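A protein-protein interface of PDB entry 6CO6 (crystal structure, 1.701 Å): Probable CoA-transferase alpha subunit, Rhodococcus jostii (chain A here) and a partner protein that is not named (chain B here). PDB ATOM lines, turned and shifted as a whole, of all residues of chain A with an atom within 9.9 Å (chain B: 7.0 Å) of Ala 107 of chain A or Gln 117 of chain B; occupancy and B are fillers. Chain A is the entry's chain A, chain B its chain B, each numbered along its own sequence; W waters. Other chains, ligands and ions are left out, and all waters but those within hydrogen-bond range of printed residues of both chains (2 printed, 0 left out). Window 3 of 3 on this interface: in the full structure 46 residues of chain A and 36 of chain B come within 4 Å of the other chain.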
ATOM      1  N   CYS A  76     -31.917 -24.739  14.284  1.00  0.00           N
ATOM      2  CA  CYS A  76     -31.448 -24.887  15.659  1.00  0.00           C
ATOM      3  C   CYS A  76     -32.409 -24.240  16.649  1.00  0.00           C
ATOM      4  O   CYS A  76     -32.600 -24.758  17.751  1.00  0.00           O
ATOM      5  CB  CYS A  76     -30.062 -24.281  15.834  1.00  0.00           C
ATOM      6  SG  CYS A  76     -28.737 -25.257  15.097  1.00  0.00           S
ATOM      7  N   TYR A  86     -20.756 -29.116   8.327  1.00  0.00           N
ATOM      8  CA  TYR A  86     -20.694 -27.778   7.745  1.00  0.00           C
ATOM      9  C   TYR A  86     -19.247 -27.335   7.619  1.00  0.00           C
ATOM     10  O   TYR A  86     -18.369 -27.801   8.348  1.00  0.00           O
ATOM     11  CB  TYR A  86     -21.486 -26.765   8.588  1.00  0.00           C
ATOM     12  CG  TYR A  86     -21.012 -26.721  10.022  1.00  0.00           C
ATOM     13  CD1 TYR A  86     -19.991 -25.866  10.408  1.00  0.00           C
ATOM     14  CD2 TYR A  86     -21.561 -27.568  10.982  1.00  0.00           C
ATOM     15  CE1 TYR A  86     -19.534 -25.844  11.715  1.00  0.00           C
ATOM     16  CE2 TYR A  86     -21.111 -27.551  12.301  1.00  0.00           C
ATOM     17  CZ  TYR A  86     -20.096 -26.686  12.651  1.00  0.00           C
ATOM     18  OH  TYR A  86     -19.640 -26.664  13.945  1.00  0.00           O
ATOM     19  N   PRO A  99     -26.974 -16.259  15.923  1.00  0.00           N
ATOM     20  CA  PRO A  99     -27.103 -16.416  17.382  1.00  0.00           C
ATOM     21  C   PRO A  99     -27.702 -17.748  17.798  1.00  0.00           C
ATOM     22  O   PRO A  99     -27.441 -18.202  18.918  1.00  0.00           O
ATOM     23  CB  PRO A  99     -28.011 -15.243  17.775  1.00  0.00           C
ATOM     24  CG  PRO A  99     -28.830 -14.977  16.550  1.00  0.00           C
ATOM     25  CD  PRO A  99     -27.901 -15.248  15.383  1.00  0.00           C
ATOM     26  N   TRP A 100     -28.488 -18.389  16.931  1.00  0.00           N
ATOM     27  CA  TRP A 100     -29.105 -19.661  17.286  1.00  0.00           C
ATOM     28  C   TRP A 100     -28.127 -20.821  17.149  1.00  0.00           C
ATOM     29  O   TRP A 100     -28.111 -21.728  17.991  1.00  0.00           O
ATOM     30  CB  TRP A 100     -30.352 -19.883  16.434  1.00  0.00           C
ATOM     31  CG  TRP A 100     -31.540 -19.128  16.958  1.00  0.00           C
ATOM     32  CD1 TRP A 100     -32.225 -18.112  16.338  1.00  0.00           C
ATOM     33  CD2 TRP A 100     -32.174 -19.323  18.225  1.00  0.00           C
ATOM     34  NE1 TRP A 100     -33.256 -17.669  17.151  1.00  0.00           N
ATOM     35  CE2 TRP A 100     -33.244 -18.401  18.310  1.00  0.00           C
ATOM     36  CE3 TRP A 100     -31.952 -20.197  19.289  1.00  0.00           C
ATOM     37  CZ2 TRP A 100     -34.078 -18.331  19.421  1.00  0.00           C
ATOM     38  CZ3 TRP A 100     -32.788 -20.126  20.392  1.00  0.00           C
ATOM     39  CH2 TRP A 100     -33.829 -19.202  20.447  1.00  0.00           C
ATOM     40  N   PHE A 101     -27.311 -20.820  16.094  1.00  0.00           N
ATOM     41  CA  PHE A 101     -26.211 -21.774  16.035  1.00  0.00           C
ATOM     42  C   PHE A 101     -25.306 -21.623  17.251  1.00  0.00           C
ATOM     43  O   PHE A 101     -24.936 -22.615  17.892  1.00  0.00           O
ATOM     44  CB  PHE A 101     -25.433 -21.574  14.732  1.00  0.00           C
ATOM     45  CG  PHE A 101     -24.247 -22.493  14.580  1.00  0.00           C
ATOM     46  CD1 PHE A 101     -24.431 -23.850  14.409  1.00  0.00           C
ATOM     47  CD2 PHE A 101     -22.953 -21.983  14.590  1.00  0.00           C
ATOM     48  CE1 PHE A 101     -23.334 -24.701  14.269  1.00  0.00           C
ATOM     49  CE2 PHE A 101     -21.858 -22.820  14.449  1.00  0.00           C
ATOM     50  CZ  PHE A 101     -22.051 -24.185  14.284  1.00  0.00           C
ATOM     51  N   ALA A 102     -24.977 -20.380  17.614  1.00  0.00           N
ATOM     52  CA  ALA A 102     -24.128 -20.154  18.777  1.00  0.00           C
ATOM     53  C   ALA A 102     -24.761 -20.737  20.039  1.00  0.00           C
ATOM     54  O   ALA A 102     -24.096 -21.441  20.808  1.00  0.00           O
ATOM     55  CB  ALA A 102     -23.853 -18.657  18.948  1.00  0.00           C
ATOM     56  N   LYS A 103     -26.058 -20.484  20.246  1.00  0.00           N
ATOM     57  CA  LYS A 103     -26.738 -21.017  21.425  1.00  0.00           C
ATOM     58  C   LYS A 103     -26.733 -22.542  21.426  1.00  0.00           C
ATOM     59  O   LYS A 103     -26.508 -23.167  22.467  1.00  0.00           O
ATOM     60  CB  LYS A 103     -28.174 -20.496  21.485  1.00  0.00           C
ATOM     61  CG  LYS A 103     -28.299 -19.046  21.949  1.00  0.00           C
ATOM     62  CD  LYS A 103     -29.731 -18.537  21.786  1.00  0.00           C
ATOM     63  CE  LYS A 103     -29.920 -17.167  22.416  1.00  0.00           C
ATOM     64  NZ  LYS A 103     -30.032 -17.265  23.903  1.00  0.00           N
ATOM     65  N   ALA A 104     -27.016 -23.158  20.274  1.00  0.00           N
ATOM     66  CA  ALA A 104     -27.022 -24.616  20.193  1.00  0.00           C
ATOM     67  C   ALA A 104     -25.645 -25.182  20.500  1.00  0.00           C
ATOM     68  O   ALA A 104     -25.518 -26.206  21.186  1.00  0.00           O
ATOM     69  CB  ALA A 104     -27.487 -25.066  18.807  1.00  0.00           C
ATOM     70  N   ARG A 105     -24.598 -24.514  20.012  1.00  0.00           N
ATOM     71  CA  ARG A 105     -23.236 -24.983  20.233  1.00  0.00           C
ATOM     72  C   ARG A 105     -22.828 -24.845  21.697  1.00  0.00           C
ATOM     73  O   ARG A 105     -22.323 -25.800  22.303  1.00  0.00           O
ATOM     74  CB  ARG A 105     -22.277 -24.204  19.330  1.00  0.00           C
ATOM     75  CG  ARG A 105     -22.403 -24.558  17.847  1.00  0.00           C
ATOM     76  CD  ARG A 105     -21.646 -25.842  17.530  1.00  0.00           C
ATOM     77  NE  ARG A 105     -20.203 -25.612  17.523  1.00  0.00           N
ATOM     78  CZ  ARG A 105     -19.304 -26.462  18.010  1.00  0.00           C
ATOM     79  NH1 ARG A 105     -19.693 -27.608  18.575  1.00  0.00           N
ATOM     80  NH2 ARG A 105     -18.012 -26.155  17.956  1.00  0.00           N
ATOM     81  N   THR A 106     -23.028 -23.664  22.285  1.00  0.00           N
ATOM     82  CA  THR A 106     -22.570 -23.470  23.656  1.00  0.00           C
ATOM     83  C   THR A 106     -23.388 -24.283  24.653  1.00  0.00           C
ATOM     84  O   THR A 106     -22.895 -24.566  25.750  1.00  0.00           O
ATOM     85  CB  THR A 106     -22.600 -21.984  24.037  1.00  0.00           C
ATOM     86  OG1 THR A 106     -23.923 -21.463  23.859  1.00  0.00           O
ATOM     87  CG2 THR A 106     -21.627 -21.189  23.176  1.00  0.00           C
ATOM     88  N   ALA A 107     -24.613 -24.670  24.292  1.00  0.00           N
ATOM     89  CA  ALA A 107     -25.434 -25.565  25.101  1.00  0.00           C
ATOM     90  C   ALA A 107     -25.166 -27.035  24.820  1.00  0.00           C
ATOM     91  O   ALA A 107     -25.746 -27.893  25.498  1.00  0.00           O
ATOM     92  CB  ALA A 107     -26.919 -25.267  24.874  1.00  0.00           C
ATOM     93  N   GLY A 108     -24.307 -27.347  23.849  1.00  0.00           N
ATOM     94  CA  GLY A 108     -24.047 -28.731  23.478  1.00  0.00           C
ATOM     95  C   GLY A 108     -25.268 -29.468  22.976  1.00  0.00           C
ATOM     96  O   GLY A 108     -25.398 -30.676  23.209  1.00  0.00           O
ATOM     97  N   GLU A 109     -26.177 -28.768  22.291  1.00  0.00           N
ATOM     98  CA  GLU A 109     -27.424 -29.354  21.810  1.00  0.00           C
ATOM     99  C   GLU A 109     -27.267 -30.108  20.499  1.00  0.00           C
ATOM    100  O   GLU A 109     -28.170 -30.862  20.121  1.00  0.00           O
ATOM    101  CB  GLU A 109     -28.484 -28.266  21.623  1.00  0.00           C
ATOM    102  CG  GLU A 109     -28.993 -27.653  22.908  1.00  0.00           C
ATOM    103  CD  GLU A 109     -29.929 -26.483  22.663  1.00  0.00           C
ATOM    104  OE1 GLU A 109     -30.107 -26.085  21.490  1.00  0.00           O
ATOM    105  OE2 GLU A 109     -30.477 -25.953  23.650  1.00  0.00           O
ATOM    106  N   ILE A 110     -26.164 -29.916  19.785  1.00  0.00           N
ATOM    107  CA  ILE A 110     -25.960 -30.581  18.511  1.00  0.00           C
ATOM    108  C   ILE A 110     -24.574 -31.206  18.503  1.00  0.00           C
ATOM    109  O   ILE A 110     -23.638 -30.698  19.131  1.00  0.00           O
ATOM    110  CB  ILE A 110     -26.126 -29.616  17.316  1.00  0.00           C
ATOM    111  CG1 ILE A 110     -25.179 -28.429  17.448  1.00  0.00           C
ATOM    112  CG2 ILE A 110     -27.572 -29.111  17.219  1.00  0.00           C
ATOM    113  CD1 ILE A 110     -25.248 -27.475  16.245  1.00  0.00           C
ATOM    114  N   ALA A 111     -24.460 -32.335  17.815  1.00  0.00           N
ATOM    115  CA  ALA A 111     -23.175 -32.922  17.480  1.00  0.00           C
ATOM    116  C   ALA A 111     -22.707 -32.283  16.181  1.00  0.00           C
ATOM    117  O   ALA A 111     -23.522 -32.039  15.289  1.00  0.00           O
ATOM    118  CB  ALA A 111     -23.302 -34.436  17.310  1.00  0.00           C
ATOM    119  N   VAL A 112     -21.418 -31.966  16.079  1.00  0.00           N
ATOM    120  CA  VAL A 112     -20.921 -31.329  14.863  1.00  0.00           C
ATOM    121  C   VAL A 112     -19.847 -32.184  14.203  1.00  0.00           C
ATOM    122  O   VAL A 112     -18.992 -32.782  14.869  1.00  0.00           O
ATOM    123  CB  VAL A 112     -20.395 -29.893  15.097  1.00  0.00           C
ATOM    124  CG1 VAL A 112     -21.507 -29.003  15.714  1.00  0.00           C
ATOM    125  CG2 VAL A 112     -19.123 -29.891  15.955  1.00  0.00           C
ATOM    126  N   GLU A 114     -17.776 -30.580  11.911  1.00  0.00           N
ATOM    127  CA  GLU A 114     -17.261 -29.390  11.259  1.00  0.00           C
ATOM    128  C   GLU A 114     -16.057 -29.793  10.407  1.00  0.00           C
ATOM    129  O   GLU A 114     -15.314 -30.720  10.747  1.00  0.00           O
ATOM    130  CB  GLU A 114     -16.921 -28.358  12.341  1.00  0.00           C
ATOM    131  CG  GLU A 114     -16.111 -27.149  11.936  1.00  0.00           C
ATOM    132  CD  GLU A 114     -16.061 -26.111  13.060  1.00  0.00           C
ATOM    133  OE1 GLU A 114     -16.995 -26.051  13.904  1.00  0.00           O
ATOM    134  OE2 GLU A 114     -15.054 -25.381  13.143  1.00  0.00           O
ATOM    135  N   PHE A 147     -12.840 -33.330  15.409  1.00  0.00           N
ATOM    136  CA  PHE A 147     -14.292 -33.179  15.279  1.00  0.00           C
ATOM    137  C   PHE A 147     -14.930 -34.488  14.832  1.00  0.00           C
ATOM    138  O   PHE A 147     -16.052 -34.814  15.237  1.00  0.00           O
ATOM    139  CB  PHE A 147     -14.637 -32.093  14.255  1.00  0.00           C
ATOM    140  CG  PHE A 147     -14.600 -30.685  14.783  1.00  0.00           C
ATOM    141  CD1 PHE A 147     -15.484 -30.271  15.763  1.00  0.00           C
ATOM    142  CD2 PHE A 147     -13.727 -29.755  14.233  1.00  0.00           C
ATOM    143  CE1 PHE A 147     -15.472 -28.961  16.221  1.00  0.00           C
ATOM    144  CE2 PHE A 147     -13.701 -28.442  14.690  1.00  0.00           C
ATOM    145  CZ  PHE A 147     -14.582 -28.047  15.684  1.00  0.00           C
ATOM    146  N   PHE B 112     -13.933 -21.031  20.815  1.00  0.00           N
ATOM    147  CA  PHE B 112     -13.187 -21.224  22.055  1.00  0.00           C
ATOM    148  C   PHE B 112     -13.841 -22.338  22.864  1.00  0.00           C
ATOM    149  O   PHE B 112     -15.064 -22.476  22.859  1.00  0.00           O
ATOM    150  CB  PHE B 112     -13.158 -19.946  22.896  1.00  0.00           C
ATOM    151  CG  PHE B 112     -12.293 -18.853  22.337  1.00  0.00           C
ATOM    152  CD1 PHE B 112     -10.951 -18.769  22.674  1.00  0.00           C
ATOM    153  CD2 PHE B 112     -12.827 -17.889  21.497  1.00  0.00           C
ATOM    154  CE1 PHE B 112     -10.153 -17.750  22.171  1.00  0.00           C
ATOM    155  CE2 PHE B 112     -12.034 -16.869  20.993  1.00  0.00           C
ATOM    156  CZ  PHE B 112     -10.697 -16.801  21.331  1.00  0.00           C
ATOM    157  N   GLY B 113     -13.026 -23.124  23.562  1.00  0.00           N
ATOM    158  CA  GLY B 113     -13.535 -24.145  24.452  1.00  0.00           C
ATOM    159  C   GLY B 113     -13.628 -25.516  23.806  1.00  0.00           C
ATOM    160  O   GLY B 113     -13.059 -25.761  22.738  1.00  0.00           O
ATOM    161  N   PRO B 114     -14.355 -26.433  24.450  1.00  0.00           N
ATOM    162  CA  PRO B 114     -14.450 -27.813  23.944  1.00  0.00           C
ATOM    163  C   PRO B 114     -15.076 -27.889  22.555  1.00  0.00           C
ATOM    164  O   PRO B 114     -16.004 -27.145  22.229  1.00  0.00           O
ATOM    165  CB  PRO B 114     -15.331 -28.509  24.992  1.00  0.00           C
ATOM    166  CG  PRO B 114     -15.166 -27.690  26.235  1.00  0.00           C
ATOM    167  CD  PRO B 114     -15.019 -26.274  25.757  1.00  0.00           C
ATOM    168  N   LEU B 115     -14.574 -28.830  21.742  1.00  0.00           N
ATOM    169  CA  LEU B 115     -14.986 -28.897  20.341  1.00  0.00           C
ATOM    170  C   LEU B 115     -16.490 -29.109  20.190  1.00  0.00           C
ATOM    171  O   LEU B 115     -17.109 -28.537  19.288  1.00  0.00           O
ATOM    172  CB  LEU B 115     -14.226 -30.010  19.610  1.00  0.00           C
ATOM    173  CG  LEU B 115     -12.877 -29.618  18.995  1.00  0.00           C
ATOM    174  CD1 LEU B 115     -11.864 -29.292  20.087  1.00  0.00           C
ATOM    175  CD2 LEU B 115     -12.359 -30.724  18.082  1.00  0.00           C
ATOM    176  N   GLN B 116     -17.091 -29.947  21.035  1.00  0.00           N
ATOM    177  CA  GLN B 116     -18.509 -30.253  20.897  1.00  0.00           C
ATOM    178  C   GLN B 116     -19.390 -29.418  21.826  1.00  0.00           C
ATOM    179  O   GLN B 116     -20.616 -29.560  21.789  1.00  0.00           O
ATOM    180  CB  GLN B 116     -18.757 -31.757  21.127  1.00  0.00           C
ATOM    181  CG  GLN B 116     -18.048 -32.677  20.068  1.00  0.00           C
ATOM    182  CD  GLN B 116     -18.659 -32.582  18.663  1.00  0.00           C
ATOM    183  OE1 GLN B 116     -19.841 -32.278  18.509  1.00  0.00           O
ATOM    184  NE2 GLN B 116     -17.846 -32.853  17.627  1.00  0.00           N
ATOM    185  N   GLN B 117     -18.799 -28.558  22.655  1.00  0.00           N
ATOM    186  CA  GLN B 117     -19.562 -27.599  23.460  1.00  0.00           C
ATOM    187  C   GLN B 117     -18.676 -26.408  23.771  1.00  0.00           C
ATOM    188  O   GLN B 117     -18.184 -26.245  24.896  1.00  0.00           O
ATOM    189  CB  GLN B 117     -20.091 -28.226  24.746  1.00  0.00           C
ATOM    190  CG  GLN B 117     -21.122 -27.342  25.428  1.00  0.00           C
ATOM    191  CD  GLN B 117     -21.829 -28.045  26.564  1.00  0.00           C
ATOM    192  OE1 GLN B 117     -21.669 -29.248  26.759  1.00  0.00           O
ATOM    193  NE2 GLN B 117     -22.629 -27.295  27.322  1.00  0.00           N
ATOM    194  N   PRO B 118     -18.446 -25.545  22.785  1.00  0.00           N
ATOM    195  CA  PRO B 118     -17.568 -24.391  22.986  1.00  0.00           C
ATOM    196  C   PRO B 118     -18.143 -23.402  23.988  1.00  0.00           C
ATOM    197  O   PRO B 118     -19.336 -23.393  24.299  1.00  0.00           O
ATOM    198  CB  PRO B 118     -17.499 -23.770  21.589  1.00  0.00           C
ATOM    199  CG  PRO B 118     -18.790 -24.150  20.966  1.00  0.00           C
ATOM    200  CD  PRO B 118     -19.014 -25.559  21.428  1.00  0.00           C
ATOM    201  N   THR B 119     -17.257 -22.558  24.499  1.00  0.00           N
ATOM    202  CA  THR B 119     -17.673 -21.458  25.351  1.00  0.00           C
ATOM    203  C   THR B 119     -17.994 -20.207  24.550  1.00  0.00           C
ATOM    204  O   THR B 119     -18.694 -19.325  25.050  1.00  0.00           O
ATOM    205  CB  THR B 119     -16.585 -21.161  26.385  1.00  0.00           C
ATOM    206  OG1 THR B 119     -15.327 -20.993  25.709  1.00  0.00           O
ATOM    207  CG2 THR B 119     -16.471 -22.321  27.349  1.00  0.00           C
ATOM    208  N   ARG B 120     -17.517 -20.125  23.313  1.00  0.00           N
ATOM    209  CA  ARG B 120     -17.798 -18.989  22.448  1.00  0.00           C
ATOM    210  C   ARG B 120     -17.674 -19.480  21.017  1.00  0.00           C
ATOM    211  O   ARG B 120     -16.684 -20.129  20.677  1.00  0.00           O
ATOM    212  CB  ARG B 120     -16.830 -17.836  22.723  1.00  0.00           C
ATOM    213  CG  ARG B 120     -16.970 -16.647  21.788  1.00  0.00           C
ATOM    214  CD  ARG B 120     -16.174 -15.460  22.314  1.00  0.00           C
ATOM    215  NE  ARG B 120     -15.161 -15.026  21.359  1.00  0.00           N
ATOM    216  CZ  ARG B 120     -15.396 -14.207  20.340  1.00  0.00           C
ATOM    217  NH1 ARG B 120     -16.615 -13.721  20.143  1.00  0.00           N
ATOM    218  NH2 ARG B 120     -14.413 -13.869  19.521  1.00  0.00           N
HETATM  219  O   HOH W   1     -20.625 -23.851  26.806  1.00  0.00           O
HETATM  220  O   HOH W   2     -22.188 -28.490  19.765  1.00  0.00           O
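Of the 9 printed residues of chain B, 5 touch a printed residue of chain A. Printed residues of chain B that touch a printed residue of chain A: Leu 115, Gln 116, Gln 117, Pro 118 and Thr 119. Hydrophobic or aromatic side chains of chain B within 4 Å of the printed part of chain A: Leu 115 and Pro 118. Along chain B the printed residues that touch a printed residue of chain A span positions 115 to 119. Hydrophobic or aromatic side chains of chain A within 4 Å of the printed part of chain B: Val 112 and Phe 147. Among the printed residues, 14 pairs touch across the chains.
O of Leu 115 of chain B lies within hydrogen-bond range of NH1 of Arg 105 of chain A. The backbone carbonyl oxygen (O) of Thr 106 of chain A is in hydrogen-bond range of the side-chain amide nitrogen (NE2) of Gln 117 of chain B, 3.2 Å away. The side-chain amide oxygen (OE1) of Gln 116 of chain B lies within hydrogen-bond range of the backbone NH (N) of Val 112 of chain A, 2.9 Å away.
The side-chain hydroxyl of Thr 106 of chain A lies within hydrogen-bond range of the backbone carbonyl oxygen of Ala 102 of chain A, at 3.1 Å. O of Lys 103 of chain A lies within hydrogen-bond range of OG1 of Thr 106 of chain A, 3.4 Å away. N of Thr 119 of chain B lies within hydrogen-bond range of O of Phe 112 of chain B (2.7 Å).
O of Arg 105 of chain A touches CA of Gln 117 of chain B, at 3.5 Å. CD of Pro 118 of chain B touches O of Arg 105 of chain A (3.4 Å). Pro 118 of chain B touches Thr 106 of chain A. Thr 106 of chain A touches Thr 119 of chain B (CG2 to O, 3.9 Å). Gln 117 of chain B touches Ala 107 of chain A (NE2 to C, 3.6 Å). Gly 108 of chain A touches Gln 116 of chain B (CA to O, 3.9 Å). Gln 117 of chain B touches Gly 108 of chain A. Ala 111 of chain A touches Gln 116 of chain B (CA to OE1, 3.5 Å). Leu 115 of chain B touches Phe 147 of chain A. Phe 147 of chain A touches Gln 116 of chain B.
Of the printed residues of chain B, Ala 107 of chain A touches Gln 117 (3.6 Å). Of chain A, only Arg 105 (3.5 Å), Thr 106 (3.2 Å), Ala 107 (3.6 Å) and Gly 108 (3.6 Å) come within 4 Å of Gln 117 of chain B. No residue of chain A comes within 4 Å of Pro 114 of chain B. Of the printed residues of chain B, Val 112 of chain A touches Gln 116. Of the printed residues of chain B, Phe 147 of chain A touches Leu 115 and Gln 116. Of the printed residues of chain A, Gln 116 of chain B touches Arg 105, Gly 108, Ala 111, Val 112 and Phe 147. Phe 101 of chain A touches none of the printed residues of chain B. The nearest residue of chain B that does not touch Ala 107 of chain A is Pro 118 of chain B (5.4 Å).
Water W1 bridges the backbone carbonyl oxygen of Thr 106 of chain A (2.6 Å) and the backbone carbonyl oxygen of Pro 118 of chain B (2.9 Å). Water W2 lies within hydrogen-bond range of O of Ile 110 of chain A, O of Gln 116 of chain B and NH1 of Arg 105 of chain A.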
